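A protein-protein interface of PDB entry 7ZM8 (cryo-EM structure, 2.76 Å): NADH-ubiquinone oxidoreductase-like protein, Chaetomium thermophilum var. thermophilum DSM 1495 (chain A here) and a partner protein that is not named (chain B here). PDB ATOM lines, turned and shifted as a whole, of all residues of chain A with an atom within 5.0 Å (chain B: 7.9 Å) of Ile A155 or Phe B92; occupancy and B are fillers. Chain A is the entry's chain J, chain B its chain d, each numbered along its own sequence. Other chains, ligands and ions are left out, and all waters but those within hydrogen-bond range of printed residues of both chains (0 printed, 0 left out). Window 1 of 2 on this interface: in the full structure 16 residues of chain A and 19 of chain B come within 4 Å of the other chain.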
ATOM      1  N   ARG A 153      12.752  13.044 -22.082  1.00  0.00           N
ATOM      2  CA  ARG A 153      12.285  13.281 -20.701  1.00  0.00           C
ATOM      3  C   ARG A 153      13.199  14.287 -20.034  1.00  0.00           C
ATOM      4  O   ARG A 153      14.288  14.499 -20.537  1.00  0.00           O
ATOM      5  CB  ARG A 153      12.291  11.966 -19.914  1.00  0.00           C
ATOM      6  CG  ARG A 153      11.069  11.087 -20.127  1.00  0.00           C
ATOM      7  CD  ARG A 153      11.250   9.786 -19.374  1.00  0.00           C
ATOM      8  NE  ARG A 153      10.067   8.940 -19.358  1.00  0.00           N
ATOM      9  CZ  ARG A 153       9.760   8.061 -20.302  1.00  0.00           C
ATOM     10  NH1 ARG A 153      10.543   7.918 -21.355  1.00  0.00           N
ATOM     11  NH2 ARG A 153       8.661   7.340 -20.198  1.00  0.00           N
ATOM     12  N   PRO A 154      12.764  14.967 -18.954  1.00  0.00           N
ATOM     13  CA  PRO A 154      13.660  15.818 -18.172  1.00  0.00           C
ATOM     14  C   PRO A 154      14.886  15.021 -17.703  1.00  0.00           C
ATOM     15  O   PRO A 154      14.744  13.882 -17.354  1.00  0.00           O
ATOM     16  CB  PRO A 154      12.801  16.116 -16.949  1.00  0.00           C
ATOM     17  CG  PRO A 154      11.402  16.142 -17.485  1.00  0.00           C
ATOM     18  CD  PRO A 154      11.380  15.003 -18.476  1.00  0.00           C
ATOM     19  N   ILE A 155      16.059  15.652 -17.678  1.00  0.00           N
ATOM     20  CA  ILE A 155      17.251  14.973 -17.188  1.00  0.00           C
ATOM     21  C   ILE A 155      17.074  14.551 -15.738  1.00  0.00           C
ATOM     22  O   ILE A 155      17.600  13.515 -15.318  1.00  0.00           O
ATOM     23  CB  ILE A 155      18.483  15.879 -17.379  1.00  0.00           C
ATOM     24  CG1 ILE A 155      19.758  15.095 -17.124  1.00  0.00           C
ATOM     25  CG2 ILE A 155      18.412  17.106 -16.482  1.00  0.00           C
ATOM     26  CD1 ILE A 155      19.960  14.013 -18.095  1.00  0.00           C
ATOM     27  N   GLU A 156      16.351  15.342 -14.958  1.00  0.00           N
ATOM     28  CA  GLU A 156      16.172  15.067 -13.511  1.00  0.00           C
ATOM     29  C   GLU A 156      15.374  13.785 -13.346  1.00  0.00           C
ATOM     30  O   GLU A 156      15.660  13.026 -12.438  1.00  0.00           O
ATOM     31  CB  GLU A 156      15.390  16.221 -12.891  1.00  0.00           C
ATOM     32  CG  GLU A 156      16.115  17.554 -12.947  1.00  0.00           C
ATOM     33  CD  GLU A 156      15.942  18.338 -14.237  1.00  0.00           C
ATOM     34  OE1 GLU A 156      15.150  17.899 -15.094  1.00  0.00           O
ATOM     35  OE2 GLU A 156      16.605  19.383 -14.382  1.00  0.00           O
ATOM     36  N   GLU A 157      14.402  13.569 -14.216  1.00  0.00           N
ATOM     37  CA  GLU A 157      13.549  12.365 -14.167  1.00  0.00           C
ATOM     38  C   GLU A 157      14.395  11.089 -14.254  1.00  0.00           C
ATOM     39  O   GLU A 157      14.117  10.161 -13.481  1.00  0.00           O
ATOM     40  CB  GLU A 157      12.517  12.462 -15.292  1.00  0.00           C
ATOM     41  CG  GLU A 157      11.534  11.306 -15.296  1.00  0.00           C
ATOM     42  CD  GLU A 157      10.328  11.469 -16.200  1.00  0.00           C
ATOM     43  OE1 GLU A 157       9.611  10.471 -16.411  1.00  0.00           O
ATOM     44  OE2 GLU A 157      10.100  12.594 -16.683  1.00  0.00           O
ATOM     45  N   THR A 158      15.357  11.022 -15.172  1.00  0.00           N
ATOM     46  CA  THR A 158      16.144   9.780 -15.365  1.00  0.00           C
ATOM     47  C   THR A 158      17.169   9.630 -14.245  1.00  0.00           C
ATOM     48  O   THR A 158      17.335   8.503 -13.772  1.00  0.00           O
ATOM     49  CB  THR A 158      16.804   9.741 -16.747  1.00  0.00           C
ATOM     50  OG1 THR A 158      15.759   9.838 -17.713  1.00  0.00           O
ATOM     51  CG2 THR A 158      17.616   8.491 -17.002  1.00  0.00           C
ATOM     52  N   LEU A 159      17.751  10.731 -13.770  1.00  0.00           N
ATOM     53  CA  LEU A 159      18.841  10.670 -12.765  1.00  0.00           C
ATOM     54  C   LEU A 159      18.248  10.213 -11.448  1.00  0.00           C
ATOM     55  O   LEU A 159      19.009   9.925 -10.519  1.00  0.00           O
ATOM     56  CB  LEU A 159      19.486  12.048 -12.628  1.00  0.00           C
ATOM     57  CG  LEU A 159      20.322  12.491 -13.826  1.00  0.00           C
ATOM     58  CD1 LEU A 159      20.937  13.858 -13.591  1.00  0.00           C
ATOM     59  CD2 LEU A 159      21.396  11.466 -14.147  1.00  0.00           C
ATOM     60  N   ILE A 162      18.190   6.007 -12.148  1.00  0.00           N
ATOM     61  CA  ILE A 162      19.512   5.350 -12.307  1.00  0.00           C
ATOM     62  C   ILE A 162      20.522   6.049 -11.400  1.00  0.00           C
ATOM     63  O   ILE A 162      21.253   5.341 -10.699  1.00  0.00           O
ATOM     64  CB  ILE A 162      19.963   5.273 -13.781  1.00  0.00           C
ATOM     65  CG1 ILE A 162      19.892   6.623 -14.498  1.00  0.00           C
ATOM     66  CG2 ILE A 162      19.185   4.196 -14.516  1.00  0.00           C
ATOM     67  CD1 ILE A 162      20.633   6.650 -15.808  1.00  0.00           C
ATOM     68  N   ILE A 168      27.269   7.655 -16.390  1.00  0.00           N
ATOM     69  CA  ILE A 168      26.245   8.720 -16.533  1.00  0.00           C
ATOM     70  C   ILE A 168      26.844   9.935 -15.851  1.00  0.00           C
ATOM     71  O   ILE A 168      26.619  10.109 -14.651  1.00  0.00           O
ATOM     72  CB  ILE A 168      24.905   8.302 -15.899  1.00  0.00           C
ATOM     73  CG1 ILE A 168      24.462   6.920 -16.385  1.00  0.00           C
ATOM     74  CG2 ILE A 168      23.837   9.353 -16.160  1.00  0.00           C
ATOM     75  CD1 ILE A 168      24.064   6.880 -17.840  1.00  0.00           C
ATOM     76  N   PHE B  20      20.158  17.464 -30.357  1.00  0.00           N
ATOM     77  CA  PHE B  20      18.790  17.002 -30.512  1.00  0.00           C
ATOM     78  C   PHE B  20      17.780  18.097 -30.230  1.00  0.00           C
ATOM     79  O   PHE B  20      16.589  17.902 -30.488  1.00  0.00           O
ATOM     80  CB  PHE B  20      18.517  15.807 -29.588  1.00  0.00           C
ATOM     81  CG  PHE B  20      19.081  14.524 -30.094  1.00  0.00           C
ATOM     82  CD1 PHE B  20      18.529  13.897 -31.193  1.00  0.00           C
ATOM     83  CD2 PHE B  20      20.171  13.948 -29.486  1.00  0.00           C
ATOM     84  CE1 PHE B  20      19.052  12.725 -31.668  1.00  0.00           C
ATOM     85  CE2 PHE B  20      20.691  12.768 -29.960  1.00  0.00           C
ATOM     86  CZ  PHE B  20      20.132  12.160 -31.052  1.00  0.00           C
ATOM     87  N   TYR B  25      11.235  14.563 -33.911  1.00  0.00           N
ATOM     88  CA  TYR B  25      11.626  13.160 -33.966  1.00  0.00           C
ATOM     89  C   TYR B  25      10.887  12.423 -35.072  1.00  0.00           C
ATOM     90  O   TYR B  25      11.470  11.568 -35.747  1.00  0.00           O
ATOM     91  CB  TYR B  25      11.393  12.491 -32.613  1.00  0.00           C
ATOM     92  CG  TYR B  25      12.494  12.755 -31.614  1.00  0.00           C
ATOM     93  CD1 TYR B  25      13.295  13.878 -31.719  1.00  0.00           C
ATOM     94  CD2 TYR B  25      12.727  11.889 -30.564  1.00  0.00           C
ATOM     95  CE1 TYR B  25      14.292  14.129 -30.810  1.00  0.00           C
ATOM     96  CE2 TYR B  25      13.724  12.133 -29.649  1.00  0.00           C
ATOM     97  CZ  TYR B  25      14.501  13.255 -29.780  1.00  0.00           C
ATOM     98  OH  TYR B  25      15.501  13.506 -28.878  1.00  0.00           O
ATOM     99  N   LYS B  88      30.227   7.671 -26.245  1.00  0.00           N
ATOM    100  CA  LYS B  88      29.151   7.318 -25.289  1.00  0.00           C
ATOM    101  C   LYS B  88      27.834   7.106 -26.017  1.00  0.00           C
ATOM    102  O   LYS B  88      26.912   6.629 -25.383  1.00  0.00           O
ATOM    103  CB  LYS B  88      29.094   8.387 -24.197  1.00  0.00           C
ATOM    104  CG  LYS B  88      30.335   8.494 -23.323  1.00  0.00           C
ATOM    105  CD  LYS B  88      30.554   7.278 -22.458  1.00  0.00           C
ATOM    106  CE  LYS B  88      29.413   7.042 -21.495  1.00  0.00           C
ATOM    107  NZ  LYS B  88      29.504   5.718 -20.841  1.00  0.00           N
ATOM    108  N   GLY B  89      27.791   7.405 -27.300  1.00  0.00           N
ATOM    109  CA  GLY B  89      26.566   7.237 -28.093  1.00  0.00           C
ATOM    110  C   GLY B  89      25.641   8.435 -28.055  1.00  0.00           C
ATOM    111  O   GLY B  89      26.039   9.451 -27.479  1.00  0.00           O
ATOM    112  N   TYR B  90      24.460   8.326 -28.670  1.00  0.00           N
ATOM    113  CA  TYR B  90      23.449   9.370 -28.653  1.00  0.00           C
ATOM    114  C   TYR B  90      22.238   9.009 -27.810  1.00  0.00           C
ATOM    115  O   TYR B  90      21.391   9.871 -27.574  1.00  0.00           O
ATOM    116  CB  TYR B  90      22.993   9.679 -30.086  1.00  0.00           C
ATOM    117  CG  TYR B  90      22.493   8.470 -30.850  1.00  0.00           C
ATOM    118  CD1 TYR B  90      21.236   7.931 -30.601  1.00  0.00           C
ATOM    119  CD2 TYR B  90      23.274   7.872 -31.819  1.00  0.00           C
ATOM    120  CE1 TYR B  90      20.786   6.838 -31.284  1.00  0.00           C
ATOM    121  CE2 TYR B  90      22.826   6.776 -32.512  1.00  0.00           C
ATOM    122  CZ  TYR B  90      21.580   6.266 -32.241  1.00  0.00           C
ATOM    123  OH  TYR B  90      21.123   5.169 -32.929  1.00  0.00           O
ATOM    124  N   LEU B  91      22.149   7.765 -27.349  1.00  0.00           N
ATOM    125  CA  LEU B  91      20.902   7.242 -26.806  1.00  0.00           C
ATOM    126  C   LEU B  91      20.469   8.008 -25.567  1.00  0.00           C
ATOM    127  O   LEU B  91      19.297   8.369 -25.428  1.00  0.00           O
ATOM    128  CB  LEU B  91      21.079   5.762 -26.493  1.00  0.00           C
ATOM    129  CG  LEU B  91      19.855   4.865 -26.423  1.00  0.00           C
ATOM    130  CD1 LEU B  91      19.097   4.911 -27.733  1.00  0.00           C
ATOM    131  CD2 LEU B  91      20.328   3.464 -26.109  1.00  0.00           C
ATOM    132  N   PHE B  92      21.400   8.253 -24.644  1.00  0.00           N
ATOM    133  CA  PHE B  92      21.090   9.108 -23.507  1.00  0.00           C
ATOM    134  C   PHE B  92      20.769  10.521 -23.968  1.00  0.00           C
ATOM    135  O   PHE B  92      19.805  11.135 -23.500  1.00  0.00           O
ATOM    136  CB  PHE B  92      22.260   9.123 -22.522  1.00  0.00           C
ATOM    137  CG  PHE B  92      21.911   9.719 -21.199  1.00  0.00           C
ATOM    138  CD1 PHE B  92      21.947  11.082 -21.014  1.00  0.00           C
ATOM    139  CD2 PHE B  92      21.507   8.919 -20.156  1.00  0.00           C
ATOM    140  CE1 PHE B  92      21.597  11.628 -19.817  1.00  0.00           C
ATOM    141  CE2 PHE B  92      21.160   9.463 -18.953  1.00  0.00           C
ATOM    142  CZ  PHE B  92      21.206  10.819 -18.781  1.00  0.00           C
ATOM    143  N   GLU B  93      21.571  11.045 -24.890  1.00  0.00           N
ATOM    144  CA  GLU B  93      21.397  12.404 -25.386  1.00  0.00           C
ATOM    145  C   GLU B  93      20.042  12.564 -26.062  1.00  0.00           C
ATOM    146  O   GLU B  93      19.366  13.581 -25.887  1.00  0.00           O
ATOM    147  CB  GLU B  93      22.532  12.710 -26.359  1.00  0.00           C
ATOM    148  CG  GLU B  93      22.579  14.087 -26.956  1.00  0.00           C
ATOM    149  CD  GLU B  93      22.846  15.155 -25.932  1.00  0.00           C
ATOM    150  OE1 GLU B  93      23.456  14.838 -24.895  1.00  0.00           O
ATOM    151  OE2 GLU B  93      22.489  16.320 -26.191  1.00  0.00           O
ATOM    152  N   GLN B  94      19.631  11.556 -26.834  1.00  0.00           N
ATOM    153  CA  GLN B  94      18.368  11.609 -27.561  1.00  0.00           C
ATOM    154  C   GLN B  94      17.163  11.564 -26.637  1.00  0.00           C
ATOM    155  O   GLN B  94      16.112  12.110 -26.976  1.00  0.00           O
ATOM    156  CB  GLN B  94      18.294  10.449 -28.549  1.00  0.00           C
ATOM    157  CG  GLN B  94      17.141  10.532 -29.514  1.00  0.00           C
ATOM    158  CD  GLN B  94      17.057   9.334 -30.418  1.00  0.00           C
ATOM    159  OE1 GLN B  94      17.228   9.450 -31.623  1.00  0.00           O
ATOM    160  NE2 GLN B  94      16.792   8.174 -29.841  1.00  0.00           N
ATOM    161  N   GLN B  95      17.286  10.916 -25.483  1.00  0.00           N
ATOM    162  CA  GLN B  95      16.147  10.592 -24.638  1.00  0.00           C
ATOM    163  C   GLN B  95      15.987  11.513 -23.444  1.00  0.00           C
ATOM    164  O   GLN B  95      15.047  11.329 -22.668  1.00  0.00           O
ATOM    165  CB  GLN B  95      16.269   9.162 -24.137  1.00  0.00           C
ATOM    166  CG  GLN B  95      16.002   8.106 -25.164  1.00  0.00           C
ATOM    167  CD  GLN B  95      16.117   6.742 -24.572  1.00  0.00           C
ATOM    168  OE1 GLN B  95      16.116   6.590 -23.355  1.00  0.00           O
ATOM    169  NE2 GLN B  95      16.213   5.733 -25.418  1.00  0.00           N
ATOM    170  N   ASN B  96      16.882  12.473 -23.262  1.00  0.00           N
ATOM    171  CA  ASN B  96      16.832  13.407 -22.152  1.00  0.00           C
ATOM    172  C   ASN B  96      17.139  14.787 -22.696  1.00  0.00           C
ATOM    173  O   ASN B  96      17.893  14.914 -23.660  1.00  0.00           O
ATOM    174  CB  ASN B  96      17.848  13.050 -21.060  1.00  0.00           C
ATOM    175  CG  ASN B  96      17.646  11.661 -20.498  1.00  0.00           C
ATOM    176  OD1 ASN B  96      16.937  11.476 -19.515  1.00  0.00           O
ATOM    177  ND2 ASN B  96      18.275  10.676 -21.118  1.00  0.00           N
ATOM    178  N   TYR B  97      16.559  15.819 -22.097  1.00  0.00           N
ATOM    179  CA  TYR B  97      16.966  17.186 -22.387  1.00  0.00           C
ATOM    180  C   TYR B  97      17.548  17.817 -21.134  1.00  0.00           C
ATOM    181  O   TYR B  97      17.024  17.627 -20.034  1.00  0.00           O
ATOM    182  CB  TYR B  97      15.815  18.029 -22.946  1.00  0.00           C
ATOM    183  CG  TYR B  97      14.465  17.847 -22.307  1.00  0.00           C
ATOM    184  CD1 TYR B  97      14.172  18.413 -21.075  1.00  0.00           C
ATOM    185  CD2 TYR B  97      13.457  17.166 -22.971  1.00  0.00           C
ATOM    186  CE1 TYR B  97      12.924  18.269 -20.501  1.00  0.00           C
ATOM    187  CE2 TYR B  97      12.207  17.010 -22.405  1.00  0.00           C
ATOM    188  CZ  TYR B  97      11.946  17.562 -21.168  1.00  0.00           C
ATOM    189  OH  TYR B  97      10.702  17.413 -20.604  1.00  0.00           O
ATOM    190  N   TRP B  98      18.658  18.526 -21.310  1.00  0.00           N
ATOM    191  CA  TRP B  98      19.353  19.227 -20.241  1.00  0.00           C
ATOM    192  C   TRP B  98      19.259  20.719 -20.516  1.00  0.00           C
ATOM    193  O   TRP B  98      19.695  21.185 -21.573  1.00  0.00           O
ATOM    194  CB  TRP B  98      20.810  18.781 -20.153  1.00  0.00           C
ATOM    195  CG  TRP B  98      21.559  19.459 -19.074  1.00  0.00           C
ATOM    196  CD1 TRP B  98      21.359  19.338 -17.736  1.00  0.00           C
ATOM    197  CD2 TRP B  98      22.622  20.394 -19.239  1.00  0.00           C
ATOM    198  NE1 TRP B  98      22.239  20.135 -17.054  1.00  0.00           N
ATOM    199  CE2 TRP B  98      23.026  20.795 -17.958  1.00  0.00           C
ATOM    200  CE3 TRP B  98      23.272  20.931 -20.351  1.00  0.00           C
ATOM    201  CZ2 TRP B  98      24.052  21.703 -17.753  1.00  0.00           C
ATOM    202  CZ3 TRP B  98      24.291  21.824 -20.149  1.00  0.00           C
ATOM    203  CH2 TRP B  98      24.674  22.207 -18.860  1.00  0.00           C
ATOM    204  N   SER B  99      18.701  21.464 -19.561  1.00  0.00           N
ATOM    205  CA  SER B  99      18.292  22.838 -19.837  1.00  0.00           C
ATOM    206  C   SER B  99      19.484  23.782 -19.918  1.00  0.00           C
ATOM    207  O   SER B  99      19.395  24.842 -20.549  1.00  0.00           O
ATOM    208  CB  SER B  99      17.306  23.315 -18.771  1.00  0.00           C
ATOM    209  OG  SER B  99      17.932  23.421 -17.505  1.00  0.00           O
ATOM    210  N   LYS B 100      20.598  23.425 -19.276  1.00  0.00           N
ATOM    211  CA  LYS B 100      21.789  24.264 -19.171  1.00  0.00           C
ATOM    212  C   LYS B 100      21.524  25.556 -18.410  1.00  0.00           C
ATOM    213  O   LYS B 100      22.227  26.551 -18.618  1.00  0.00           O
ATOM    214  CB  LYS B 100      22.383  24.596 -20.545  1.00  0.00           C
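Ile A155 touches just these residues of chain B: Phe B92, Asn B96, Tyr B97 and Trp B98. Glu A157 touches none of the printed residues of chain B. Of the printed residues of chain B, Ile A168 touches Phe B92. Printed residues of chain A within 4 Å of Gln B95: Arg A153 (2.9 Å). The nearest printed residue of chain A that does not touch Tyr B97 is Glu A156 (5.3 Å).
O of Arg A153 touches CA of Asn B96, 3.2 Å away. Pro A154 touches Asn B96 (O to OD1, 3.9 Å). Tyr B97 touches Pro A154 (OH to CD, 3.3 Å). Ile A155 touches Phe B92. Ile A155 touches Asn B96 (CD1 to CB, 3.8 Å). Trp B98 touches Ile A155 (CD1 to CG2, 3.9 Å). CG2 of Ile A168 touches CE2 of Phe B92 (3.9 Å).
Of the 15 printed residues of chain B, 5 touch a printed residue of chain A. Among the printed residues, 11 pairs touch across the chains. Among the printed residues, no Asp or Glu carboxylate lies within 4 Å of a Lys or Arg side-chain nitrogen of the other chain.
The backbone NH of Arg A153 lies within hydrogen-bond range of the backbone carbonyl oxygen of Gln B95 (2.9 Å). OG1 of Thr A158 sits at hydrogen-bond distance from OD1 of Asn B96. The backbone carbonyl oxygen (O) of Tyr B97 lies within hydrogen-bond range of the backbone NH (N) of Ile A155 (3.2 Å). O of Arg A153 sits at hydrogen-bond distance from N of Tyr B97, at 3.1 Å.
ND2 of Asn B96 lies within hydrogen-bond range of O of Phe B92 (2.9 Å). NE of Arg A153 lies within salt-bridge range of OE1 of Glu A157, at 3.4 Å.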
